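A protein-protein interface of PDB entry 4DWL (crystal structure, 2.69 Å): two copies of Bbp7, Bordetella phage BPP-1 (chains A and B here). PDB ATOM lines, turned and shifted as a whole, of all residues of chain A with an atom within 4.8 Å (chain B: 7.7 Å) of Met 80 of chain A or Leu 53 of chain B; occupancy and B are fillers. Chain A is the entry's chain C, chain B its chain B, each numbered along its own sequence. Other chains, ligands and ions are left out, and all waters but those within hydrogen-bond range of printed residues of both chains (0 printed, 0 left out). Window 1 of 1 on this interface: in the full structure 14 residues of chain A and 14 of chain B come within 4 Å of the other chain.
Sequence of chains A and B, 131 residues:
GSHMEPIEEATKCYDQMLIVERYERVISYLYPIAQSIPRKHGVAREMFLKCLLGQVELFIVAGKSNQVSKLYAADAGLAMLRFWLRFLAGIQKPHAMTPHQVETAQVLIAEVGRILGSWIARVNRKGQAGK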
ATOM      1  N   ALA A  44      11.901   0.472  17.818  1.00  0.00           N
ATOM      2  CA  ALA A  44      11.568   0.941  16.476  1.00  0.00           C
ATOM      3  C   ALA A  44      11.339  -0.255  15.556  1.00  0.00           C
ATOM      4  O   ALA A  44      10.356  -0.302  14.831  1.00  0.00           O
ATOM      5  CB  ALA A  44      12.676   1.853  15.908  1.00  0.00           C
ATOM      6  N   MET A  47       7.990  -1.919  16.336  1.00  0.00           N
ATOM      7  CA  MET A  47       6.822  -1.139  15.943  1.00  0.00           C
ATOM      8  C   MET A  47       6.643  -1.229  14.440  1.00  0.00           C
ATOM      9  O   MET A  47       5.523  -1.267  13.934  1.00  0.00           O
ATOM     10  CB  MET A  47       6.967   0.311  16.354  1.00  0.00           C
ATOM     11  CG  MET A  47       7.002   0.544  17.838  1.00  0.00           C
ATOM     12  SD  MET A  47       7.142   2.464  18.101  1.00  0.00           S
ATOM     13  CE  MET A  47       5.443   3.016  17.310  1.00  0.00           C
ATOM     14  N   CYS A  51       3.700  -2.717  12.150  1.00  0.00           N
ATOM     15  CA  CYS A  51       3.043  -1.885  11.150  1.00  0.00           C
ATOM     16  C   CYS A  51       3.058  -2.577   9.803  1.00  0.00           C
ATOM     17  O   CYS A  51       2.036  -2.619   9.105  1.00  0.00           O
ATOM     18  CB  CYS A  51       3.745  -0.535  11.042  1.00  0.00           C
ATOM     19  SG  CYS A  51       3.359   0.369   9.553  1.00  0.00           S
ATOM     20  N   ALA A  76      -3.719   5.322   5.172  1.00  0.00           N
ATOM     21  CA  ALA A  76      -2.962   5.807   6.315  1.00  0.00           C
ATOM     22  C   ALA A  76      -1.872   4.812   6.696  1.00  0.00           C
ATOM     23  O   ALA A  76      -0.743   5.194   7.013  1.00  0.00           O
ATOM     24  CB  ALA A  76      -3.893   6.040   7.474  1.00  0.00           C
ATOM     25  N   GLY A  77      -2.215   3.529   6.649  1.00  0.00           N
ATOM     26  CA  GLY A  77      -1.282   2.469   6.976  1.00  0.00           C
ATOM     27  C   GLY A  77      -0.109   2.462   6.027  1.00  0.00           C
ATOM     28  O   GLY A  77       1.028   2.275   6.452  1.00  0.00           O
ATOM     29  N   LEU A  78      -0.380   2.685   4.742  1.00  0.00           N
ATOM     30  CA  LEU A  78       0.678   2.783   3.747  1.00  0.00           C
ATOM     31  C   LEU A  78       1.553   4.024   3.950  1.00  0.00           C
ATOM     32  O   LEU A  78       2.785   3.948   3.883  1.00  0.00           O
ATOM     33  CB  LEU A  78       0.093   2.792   2.339  1.00  0.00           C
ATOM     34  CG  LEU A  78      -0.320   1.457   1.741  1.00  0.00           C
ATOM     35  CD1 LEU A  78      -0.661   1.666   0.282  1.00  0.00           C
ATOM     36  CD2 LEU A  78       0.771   0.421   1.916  1.00  0.00           C
ATOM     37  N   ALA A  79       0.921   5.170   4.188  1.00  0.00           N
ATOM     38  CA  ALA A  79       1.680   6.397   4.448  1.00  0.00           C
ATOM     39  C   ALA A  79       2.558   6.241   5.679  1.00  0.00           C
ATOM     40  O   ALA A  79       3.662   6.769   5.717  1.00  0.00           O
ATOM     41  CB  ALA A  79       0.757   7.613   4.591  1.00  0.00           C
ATOM     42  N   MET A  80       2.069   5.492   6.670  1.00  0.00           N
ATOM     43  CA  MET A  80       2.841   5.191   7.872  1.00  0.00           C
ATOM     44  C   MET A  80       4.043   4.307   7.560  1.00  0.00           C
ATOM     45  O   MET A  80       5.111   4.452   8.151  1.00  0.00           O
ATOM     46  CB  MET A  80       1.969   4.497   8.910  1.00  0.00           C
ATOM     47  CG  MET A  80       2.669   4.341  10.230  1.00  0.00           C
ATOM     48  SD  MET A  80       3.144   6.099  10.957  1.00  0.00           S
ATOM     49  CE  MET A  80       4.474   5.504  12.221  1.00  0.00           C
ATOM     50  N   LEU A  81       3.870   3.385   6.622  1.00  0.00           N
ATOM     51  CA  LEU A  81       4.942   2.472   6.283  1.00  0.00           C
ATOM     52  C   LEU A  81       6.048   3.228   5.554  1.00  0.00           C
ATOM     53  O   LEU A  81       7.224   2.932   5.725  1.00  0.00           O
ATOM     54  CB  LEU A  81       4.394   1.323   5.451  1.00  0.00           C
ATOM     55  CG  LEU A  81       5.331   0.156   5.205  1.00  0.00           C
ATOM     56  CD1 LEU A  81       5.871  -0.339   6.501  1.00  0.00           C
ATOM     57  CD2 LEU A  81       4.562  -0.921   4.531  1.00  0.00           C
ATOM     58  N   ARG A  82       5.678   4.233   4.766  1.00  0.00           N
ATOM     59  CA  ARG A  82       6.686   5.079   4.112  1.00  0.00           C
ATOM     60  C   ARG A  82       7.457   5.956   5.108  1.00  0.00           C
ATOM     61  O   ARG A  82       8.681   6.114   4.986  1.00  0.00           O
ATOM     62  CB  ARG A  82       6.068   5.933   3.001  1.00  0.00           C
ATOM     63  CG  ARG A  82       5.574   5.121   1.820  1.00  0.00           C
ATOM     64  CD  ARG A  82       5.012   6.016   0.745  1.00  0.00           C
ATOM     65  NE  ARG A  82       3.870   6.812   1.207  1.00  0.00           N
ATOM     66  CZ  ARG A  82       2.598   6.590   0.864  1.00  0.00           C
ATOM     67  NH1 ARG A  82       2.291   5.579   0.038  1.00  0.00           N
ATOM     68  NH2 ARG A  82       1.635   7.397   1.332  1.00  0.00           N
ATOM     69  N   PHE A  83       6.746   6.525   6.085  1.00  0.00           N
ATOM     70  CA  PHE A  83       7.421   7.182   7.196  1.00  0.00           C
ATOM     71  C   PHE A  83       8.463   6.261   7.837  1.00  0.00           C
ATOM     72  O   PHE A  83       9.573   6.690   8.158  1.00  0.00           O
ATOM     73  CB  PHE A  83       6.461   7.633   8.288  1.00  0.00           C
ATOM     74  CG  PHE A  83       7.150   7.839   9.620  1.00  0.00           C
ATOM     75  CD1 PHE A  83       7.873   8.997   9.867  1.00  0.00           C
ATOM     76  CD2 PHE A  83       7.119   6.861  10.598  1.00  0.00           C
ATOM     77  CE1 PHE A  83       8.526   9.181  11.065  1.00  0.00           C
ATOM     78  CE2 PHE A  83       7.775   7.043  11.797  1.00  0.00           C
ATOM     79  CZ  PHE A  83       8.482   8.211  12.026  1.00  0.00           C
ATOM     80  N   TRP A  84       8.103   5.000   8.049  1.00  0.00           N
ATOM     81  CA  TRP A  84       9.067   4.080   8.635  1.00  0.00           C
ATOM     82  C   TRP A  84      10.319   3.905   7.773  1.00  0.00           C
ATOM     83  O   TRP A  84      11.404   3.657   8.308  1.00  0.00           O
ATOM     84  CB  TRP A  84       8.444   2.733   8.984  1.00  0.00           C
ATOM     85  CG  TRP A  84       7.639   2.744  10.245  1.00  0.00           C
ATOM     86  CD1 TRP A  84       6.284   2.636  10.350  1.00  0.00           C
ATOM     87  CD2 TRP A  84       8.132   2.866  11.584  1.00  0.00           C
ATOM     88  NE1 TRP A  84       5.902   2.677  11.669  1.00  0.00           N
ATOM     89  CE2 TRP A  84       7.018   2.815  12.446  1.00  0.00           C
ATOM     90  CE3 TRP A  84       9.407   3.002  12.137  1.00  0.00           C
ATOM     91  CZ2 TRP A  84       7.135   2.899  13.826  1.00  0.00           C
ATOM     92  CZ3 TRP A  84       9.527   3.083  13.525  1.00  0.00           C
ATOM     93  CH2 TRP A  84       8.396   3.028  14.349  1.00  0.00           C
ATOM     94  N   PHE A  87      12.363   7.182   8.271  1.00  0.00           N
ATOM     95  CA  PHE A  87      12.903   7.112   9.620  1.00  0.00           C
ATOM     96  C   PHE A  87      14.073   6.133   9.713  1.00  0.00           C
ATOM     97  O   PHE A  87      15.152   6.490  10.190  1.00  0.00           O
ATOM     98  CB  PHE A  87      11.818   6.721  10.626  1.00  0.00           C
ATOM     99  CG  PHE A  87      12.341   6.518  12.006  1.00  0.00           C
ATOM    100  CD1 PHE A  87      12.474   7.605  12.874  1.00  0.00           C
ATOM    101  CD2 PHE A  87      12.733   5.254  12.435  1.00  0.00           C
ATOM    102  CE1 PHE A  87      12.978   7.434  14.153  1.00  0.00           C
ATOM    103  CE2 PHE A  87      13.239   5.071  13.708  1.00  0.00           C
ATOM    104  CZ  PHE A  87      13.358   6.160  14.576  1.00  0.00           C
ATOM    105  N   TYR B  23       7.107  17.661  12.455  1.00  0.00           N
ATOM    106  CA  TYR B  23       7.210  16.682  13.525  1.00  0.00           C
ATOM    107  C   TYR B  23       8.436  15.759  13.428  1.00  0.00           C
ATOM    108  O   TYR B  23       8.957  15.323  14.456  1.00  0.00           O
ATOM    109  CB  TYR B  23       5.929  15.885  13.711  1.00  0.00           C
ATOM    110  CG  TYR B  23       5.972  15.058  14.961  1.00  0.00           C
ATOM    111  CD1 TYR B  23       5.762  15.638  16.205  1.00  0.00           C
ATOM    112  CD2 TYR B  23       6.256  13.699  14.905  1.00  0.00           C
ATOM    113  CE1 TYR B  23       5.819  14.879  17.350  1.00  0.00           C
ATOM    114  CE2 TYR B  23       6.303  12.931  16.041  1.00  0.00           C
ATOM    115  CZ  TYR B  23       6.082  13.513  17.259  1.00  0.00           C
ATOM    116  OH  TYR B  23       6.140  12.731  18.398  1.00  0.00           O
ATOM    117  N   ILE B  27      11.167  14.221  16.293  1.00  0.00           N
ATOM    118  CA  ILE B  27      11.657  12.850  16.360  1.00  0.00           C
ATOM    119  C   ILE B  27      13.178  12.851  16.284  1.00  0.00           C
ATOM    120  O   ILE B  27      13.847  12.141  17.017  1.00  0.00           O
ATOM    121  CB  ILE B  27      11.066  11.966  15.229  1.00  0.00           C
ATOM    122  CG1 ILE B  27       9.565  11.773  15.422  1.00  0.00           C
ATOM    123  CG2 ILE B  27      11.717  10.630  15.222  1.00  0.00           C
ATOM    124  CD1 ILE B  27       8.860  11.356  14.194  1.00  0.00           C
ATOM    125  N   SER B  28      13.713  13.660  15.385  1.00  0.00           N
ATOM    126  CA  SER B  28      15.155  13.775  15.207  1.00  0.00           C
ATOM    127  C   SER B  28      15.841  14.204  16.498  1.00  0.00           C
ATOM    128  O   SER B  28      16.905  13.688  16.838  1.00  0.00           O
ATOM    129  CB  SER B  28      15.470  14.775  14.084  1.00  0.00           C
ATOM    130  OG  SER B  28      16.655  14.407  13.383  1.00  0.00           O
ATOM    131  N   TYR B  31      14.505  11.260  19.627  1.00  0.00           N
ATOM    132  CA  TYR B  31      14.833   9.838  19.441  1.00  0.00           C
ATOM    133  C   TYR B  31      16.159   9.405  20.071  1.00  0.00           C
ATOM    134  O   TYR B  31      16.155   8.457  20.851  1.00  0.00           O
ATOM    135  CB  TYR B  31      14.750   9.373  17.976  1.00  0.00           C
ATOM    136  CG  TYR B  31      15.000   7.875  17.820  1.00  0.00           C
ATOM    137  CD1 TYR B  31      14.025   6.946  18.163  1.00  0.00           C
ATOM    138  CD2 TYR B  31      16.201   7.392  17.328  1.00  0.00           C
ATOM    139  CE1 TYR B  31      14.242   5.589  18.028  1.00  0.00           C
ATOM    140  CE2 TYR B  31      16.423   6.026  17.190  1.00  0.00           C
ATOM    141  CZ  TYR B  31      15.440   5.133  17.544  1.00  0.00           C
ATOM    142  OH  TYR B  31      15.657   3.779  17.415  1.00  0.00           O
ATOM    143  N   GLU B  46      10.108   2.362  26.505  1.00  0.00           N
ATOM    144  CA  GLU B  46       9.236   1.867  25.434  1.00  0.00           C
ATOM    145  C   GLU B  46       7.960   2.705  25.261  1.00  0.00           C
ATOM    146  O   GLU B  46       7.584   3.050  24.134  1.00  0.00           O
ATOM    147  CB  GLU B  46       8.893   0.379  25.605  1.00  0.00           C
ATOM    148  CG  GLU B  46       8.378  -0.267  24.322  1.00  0.00           C
ATOM    149  CD  GLU B  46       7.948  -1.737  24.481  1.00  0.00           C
ATOM    150  OE1 GLU B  46       8.701  -2.526  25.094  1.00  0.00           O
ATOM    151  OE2 GLU B  46       6.854  -2.105  23.980  1.00  0.00           O
ATOM    152  N   MET B  47       7.307   3.064  26.362  1.00  0.00           N
ATOM    153  CA  MET B  47       6.075   3.847  26.252  1.00  0.00           C
ATOM    154  C   MET B  47       6.347   5.227  25.663  1.00  0.00           C
ATOM    155  O   MET B  47       5.519   5.780  24.921  1.00  0.00           O
ATOM    156  CB  MET B  47       5.382   4.004  27.595  1.00  0.00           C
ATOM    157  CG  MET B  47       4.762   2.757  28.127  1.00  0.00           C
ATOM    158  SD  MET B  47       4.045   3.143  29.906  1.00  0.00           S
ATOM    159  CE  MET B  47       2.469   4.140  29.340  1.00  0.00           C
ATOM    160  N   PHE B  48       7.507   5.778  26.016  1.00  0.00           N
ATOM    161  CA  PHE B  48       7.932   7.066  25.491  1.00  0.00           C
ATOM    162  C   PHE B  48       8.075   6.941  23.973  1.00  0.00           C
ATOM    163  O   PHE B  48       7.433   7.684  23.222  1.00  0.00           O
ATOM    164  CB  PHE B  48       9.254   7.499  26.135  1.00  0.00           C
ATOM    165  CG  PHE B  48       9.847   8.764  25.556  1.00  0.00           C
ATOM    166  CD1 PHE B  48       9.042   9.814  25.174  1.00  0.00           C
ATOM    167  CD2 PHE B  48      11.218   8.917  25.459  1.00  0.00           C
ATOM    168  CE1 PHE B  48       9.584  10.991  24.681  1.00  0.00           C
ATOM    169  CE2 PHE B  48      11.765  10.094  24.980  1.00  0.00           C
ATOM    170  CZ  PHE B  48      10.945  11.131  24.590  1.00  0.00           C
ATOM    171  N   LEU B  49       8.907   5.986  23.544  1.00  0.00           N
ATOM    172  CA  LEU B  49       9.194   5.761  22.132  1.00  0.00           C
ATOM    173  C   LEU B  49       7.902   5.569  21.350  1.00  0.00           C
ATOM    174  O   LEU B  49       7.681   6.258  20.357  1.00  0.00           O
ATOM    175  CB  LEU B  49      10.130   4.568  21.957  1.00  0.00           C
ATOM    176  CG  LEU B  49      11.616   4.914  22.025  1.00  0.00           C
ATOM    177  CD1 LEU B  49      12.430   3.645  22.118  1.00  0.00           C
ATOM    178  CD2 LEU B  49      12.026   5.720  20.812  1.00  0.00           C
ATOM    179  N   LYS B  50       7.031   4.682  21.825  1.00  0.00           N
ATOM    180  CA  LYS B  50       5.743   4.487  21.169  1.00  0.00           C
ATOM    181  C   LYS B  50       4.966   5.795  21.052  1.00  0.00           C
ATOM    182  O   LYS B  50       4.310   6.027  20.030  1.00  0.00           O
ATOM    183  CB  LYS B  50       4.887   3.427  21.868  1.00  0.00           C
ATOM    184  CG  LYS B  50       5.421   1.998  21.764  1.00  0.00           C
ATOM    185  CD  LYS B  50       4.382   1.011  22.278  1.00  0.00           C
ATOM    186  CE  LYS B  50       4.870  -0.440  22.251  1.00  0.00           C
ATOM    187  NZ  LYS B  50       3.754  -1.419  22.603  1.00  0.00           N
ATOM    188  N   CYS B  51       5.053   6.653  22.070  1.00  0.00           N
ATOM    189  CA  CYS B  51       4.332   7.927  22.048  1.00  0.00           C
ATOM    190  C   CYS B  51       4.928   8.826  20.996  1.00  0.00           C
ATOM    191  O   CYS B  51       4.210   9.522  20.288  1.00  0.00           O
ATOM    192  CB  CYS B  51       4.415   8.643  23.396  1.00  0.00           C
ATOM    193  SG  CYS B  51       3.683  10.302  23.423  1.00  0.00           S
ATOM    194  N   LEU B  52       6.257   8.802  20.915  1.00  0.00           N
ATOM    195  CA  LEU B  52       7.022   9.694  20.059  1.00  0.00           C
ATOM    196  C   LEU B  52       6.901   9.341  18.572  1.00  0.00           C
ATOM    197  O   LEU B  52       6.686  10.226  17.744  1.00  0.00           O
ATOM    198  CB  LEU B  52       8.492   9.690  20.485  1.00  0.00           C
ATOM    199  CG  LEU B  52       9.495  10.386  19.575  1.00  0.00           C
ATOM    200  CD1 LEU B  52       9.390  11.897  19.711  1.00  0.00           C
ATOM    201  CD2 LEU B  52      10.896   9.912  19.889  1.00  0.00           C
ATOM    202  N   LEU B  53       7.043   8.057  18.230  1.00  0.00           N
ATOM    203  CA  LEU B  53       6.939   7.636  16.832  1.00  0.00           C
ATOM    204  C   LEU B  53       5.481   7.478  16.433  1.00  0.00           C
ATOM    205  O   LEU B  53       5.088   7.828  15.324  1.00  0.00           O
ATOM    206  CB  LEU B  53       7.705   6.340  16.591  1.00  0.00           C
ATOM    207  CG  LEU B  53       9.158   6.428  17.058  1.00  0.00           C
ATOM    208  CD1 LEU B  53       9.814   5.048  17.100  1.00  0.00           C
ATOM    209  CD2 LEU B  53       9.973   7.418  16.213  1.00  0.00           C
ATOM    210  N   GLY B  54       4.675   6.971  17.354  1.00  0.00           N
ATOM    211  CA  GLY B  54       3.264   6.812  17.092  1.00  0.00           C
ATOM    212  C   GLY B  54       2.576   8.098  16.689  1.00  0.00           C
ATOM    213  O   GLY B  54       1.604   8.064  15.938  1.00  0.00           O
ATOM    214  N   GLN B  55       3.071   9.234  17.178  1.00  0.00           N
ATOM    215  CA  GLN B  55       2.430  10.512  16.905  1.00  0.00           C
ATOM    216  C   GLN B  55       2.306  10.776  15.388  1.00  0.00           C
ATOM    217  O   GLN B  55       1.375  11.454  14.942  1.00  0.00           O
ATOM    218  CB  GLN B  55       3.217  11.635  17.558  1.00  0.00           C
ATOM    219  CG  GLN B  55       2.615  13.005  17.348  1.00  0.00           C
ATOM    220  CD  GLN B  55       1.354  13.201  18.175  1.00  0.00           C
ATOM    221  OE1 GLN B  55       1.195  12.615  19.257  1.00  0.00           O
ATOM    222  NE2 GLN B  55       0.455  14.033  17.674  1.00  0.00           N
ATOM    223  N   VAL B  56       3.235  10.250  14.591  1.00  0.00           N
ATOM    224  CA  VAL B  56       3.138  10.428  13.151  1.00  0.00           C
ATOM    225  C   VAL B  56       1.855   9.768  12.657  1.00  0.00           C
ATOM    226  O   VAL B  56       1.106  10.334  11.852  1.00  0.00           O
ATOM    227  CB  VAL B  56       4.375   9.870  12.400  1.00  0.00           C
ATOM    228  CG1 VAL B  56       4.126   9.847  10.919  1.00  0.00           C
ATOM    229  CG2 VAL B  56       5.609  10.727  12.691  1.00  0.00           C
ATOM    230  N   GLU B  57       1.566   8.586  13.190  1.00  0.00           N
ATOM    231  CA  GLU B  57       0.386   7.888  12.738  1.00  0.00           C
ATOM    232  C   GLU B  57      -0.887   8.652  13.059  1.00  0.00           C
ATOM    233  O   GLU B  57      -1.806   8.699  12.229  1.00  0.00           O
ATOM    234  CB  GLU B  57       0.326   6.480  13.283  1.00  0.00           C
ATOM    235  CG  GLU B  57      -0.972   5.770  12.942  1.00  0.00           C
ATOM    236  CD  GLU B  57      -0.975   4.349  13.444  1.00  0.00           C
ATOM    237  OE1 GLU B  57      -0.588   4.145  14.620  1.00  0.00           O
ATOM    238  OE2 GLU B  57      -1.323   3.445  12.654  1.00  0.00           O
ATOM    239  N   LEU B  58      -0.941   9.275  14.237  1.00  0.00           N
ATOM    240  CA  LEU B  58      -2.068  10.153  14.549  1.00  0.00           C
ATOM    241  C   LEU B  58      -2.219  11.317  13.528  1.00  0.00           C
ATOM    242  O   LEU B  58      -3.339  11.714  13.207  1.00  0.00           O
ATOM    243  CB  LEU B  58      -1.972  10.676  15.977  1.00  0.00           C
ATOM    244  CG  LEU B  58      -1.979   9.659  17.118  1.00  0.00           C
ATOM    245  CD1 LEU B  58      -1.684  10.374  18.431  1.00  0.00           C
ATOM    246  CD2 LEU B  58      -3.306   8.995  17.184  1.00  0.00           C
ATOM    247  N   PHE B  59      -1.111  11.851  13.007  1.00  0.00           N
ATOM    248  CA  PHE B  59      -1.210  12.946  12.040  1.00  0.00           C
ATOM    249  C   PHE B  59      -1.684  12.432  10.692  1.00  0.00           C
ATOM    250  O   PHE B  59      -2.640  12.965  10.114  1.00  0.00           O
ATOM    251  CB  PHE B  59       0.120  13.684  11.881  1.00  0.00           C
ATOM    252  CG  PHE B  59       0.442  14.584  13.030  1.00  0.00           C
ATOM    253  CD1 PHE B  59      -0.526  15.416  13.561  1.00  0.00           C
ATOM    254  CD2 PHE B  59       1.701  14.581  13.603  1.00  0.00           C
ATOM    255  CE1 PHE B  59      -0.239  16.233  14.639  1.00  0.00           C
ATOM    256  CE2 PHE B  59       1.984  15.390  14.677  1.00  0.00           C
ATOM    257  CZ  PHE B  59       1.015  16.220  15.187  1.00  0.00           C
ATOM    258  N   ILE B  60      -1.005  11.386  10.214  1.00  0.00           N
ATOM    259  CA  ILE B  60      -1.338  10.710   8.962  1.00  0.00           C
ATOM    260  C   ILE B  60      -2.809  10.300   8.932  1.00  0.00           C
ATOM    261  O   ILE B  60      -3.508  10.557   7.963  1.00  0.00           O
ATOM    262  CB  ILE B  60      -0.454   9.458   8.758  1.00  0.00           C
ATOM    263  CG1 ILE B  60       0.995   9.862   8.512  1.00  0.00           C
ATOM    264  CG2 ILE B  60      -0.958   8.608   7.611  1.00  0.00           C
ATOM    265  CD1 ILE B  60       1.874   8.702   8.195  1.00  0.00           C
ATOM    266  N   VAL B  61      -3.281   9.681  10.009  1.00  0.00           N
ATOM    267  CA  VAL B  61      -4.662   9.221  10.079  1.00  0.00           C
ATOM    268  C   VAL B  61      -5.642  10.382   9.999  1.00  0.00           C
ATOM    269  O   VAL B  61      -6.617  10.322   9.260  1.00  0.00           O
ATOM    270  CB  VAL B  61      -4.923   8.372  11.359  1.00  0.00           C
ATOM    271  CG1 VAL B  61      -6.342   8.562  11.864  1.00  0.00           C
ATOM    272  CG2 VAL B  61      -4.627   6.915  11.088  1.00  0.00           C
ATOM    273  N   LYS B  64      -5.690  11.509   6.318  1.00  0.00           N
ATOM    274  CA  LYS B  64      -6.480  10.605   5.485  1.00  0.00           C
ATOM    275  C   LYS B  64      -7.860  10.306   6.089  1.00  0.00           C
ATOM    276  O   LYS B  64      -8.256   9.142   6.187  1.00  0.00           O
ATOM    277  CB  LYS B  64      -5.744   9.267   5.327  1.00  0.00           C
ATOM    278  CG  LYS B  64      -4.299   9.356   4.904  1.00  0.00           C
ATOM    279  CD  LYS B  64      -4.162   9.871   3.485  1.00  0.00           C
ATOM    280  CE  LYS B  64      -2.697   9.923   3.055  1.00  0.00           C
ATOM    281  NZ  LYS B  64      -2.364   8.849   2.070  1.00  0.00           N
ATOM    282  N   LEU B  81       3.210  13.709  24.892  1.00  0.00           N
ATOM    283  CA  LEU B  81       4.639  13.783  24.638  1.00  0.00           C
ATOM    284  C   LEU B  81       5.299  14.783  25.586  1.00  0.00           C
ATOM    285  O   LEU B  81       6.422  14.576  26.032  1.00  0.00           O
ATOM    286  CB  LEU B  81       4.898  14.210  23.197  1.00  0.00           C
ATOM    287  CG  LEU B  81       6.346  14.111  22.727  1.00  0.00           C
ATOM    288  CD1 LEU B  81       6.734  12.662  22.637  1.00  0.00           C
ATOM    289  CD2 LEU B  81       6.538  14.800  21.384  1.00  0.00           C
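The side-chain sulfur of Met 80 of chain A lies close to the backbone NH of Glu 57 of chain B, at 3.7 Å.
The side-chain carboxylate (OE2) of Glu 46 of chain B lies within salt-bridge range of the side-chain amino group (NZ) of Lys 50 of chain B (3.5 Å).
Among the printed residues, pairs that only touch across the chains: Ala 44 of chain A with Tyr 31 of chain B (3.9 Å), Met 47 of chain A with Lys 50 of chain B (3.9 Å), Met 47 of chain A with Leu 53 of chain B (3.8 Å), Ala 76 of chain A with Ile 60 of chain B (3.5 Å), Ala 76 of chain A with Val 61 of chain B (3.8 Å), Ala 79 of chain A with Ile 60 of chain B (3.6 Å), Met 80 of chain A with Leu 53 of chain B (3.9 Å), Met 80 of chain A with Val 56 of chain B (3.9 Å), Met 80 of chain A with Ile 60 of chain B (3.6 Å), Phe 83 of chain A with Ile 27 of chain B (3.8 Å), Phe 83 of chain A with Val 56 of chain B (3.7 Å), Trp 84 of chain A with Leu 53 of chain B (3.7 Å), Phe 87 of chain A with Ile 27 of chain B (3.6 Å), Phe 87 of chain A with Tyr 31 of chain B (3.6 Å) and Phe 87 of chain A with Leu 53 of chain B (3.6 Å).
Of chain B, only Leu 53 (3.9 Å), Val 56 (3.9 Å), Glu 57 (3.7 Å) and Ile 60 (3.6 Å) come within 4 Å of Met 80 of chain A.
Leu 53 of chain B touches four residues of chain A.
Printed residues of chain A within 4 Å of Glu 57 of chain B: Met 80.
Of the printed residues of chain B, Ala 76 of chain A touches Ile 60 (3.5 Å) and Val 61 (3.8 Å).
Phe 59 of chain B touches none of the printed residues of chain A.
The nearest residue of chain B that does not touch Met 80 of chain A is Gly 54 of chain B (5.2 Å).
The nearest residue of chain A that does not touch Leu 53 of chain B is Ala 44 of chain A (4.5 Å).
Hydrophobic or aromatic side chains of chain B that line the printed part of chain A: Ile 27, Tyr 31, Leu 53, Val 56, Ile 60 and Val 61.
Along chain B the printed residues that touch a printed residue of chain A span positions 27 to 61.
Of the 13 printed residues of chain A, 8 touch a printed residue of chain B.
Among the printed residues, 16 pairs touch across the chains.
Among the printed residues, no Asp or Glu carboxylate lies within 4 Å of a Lys or Arg side-chain nitrogen of the other chain.
3 positions are printed for both chains.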
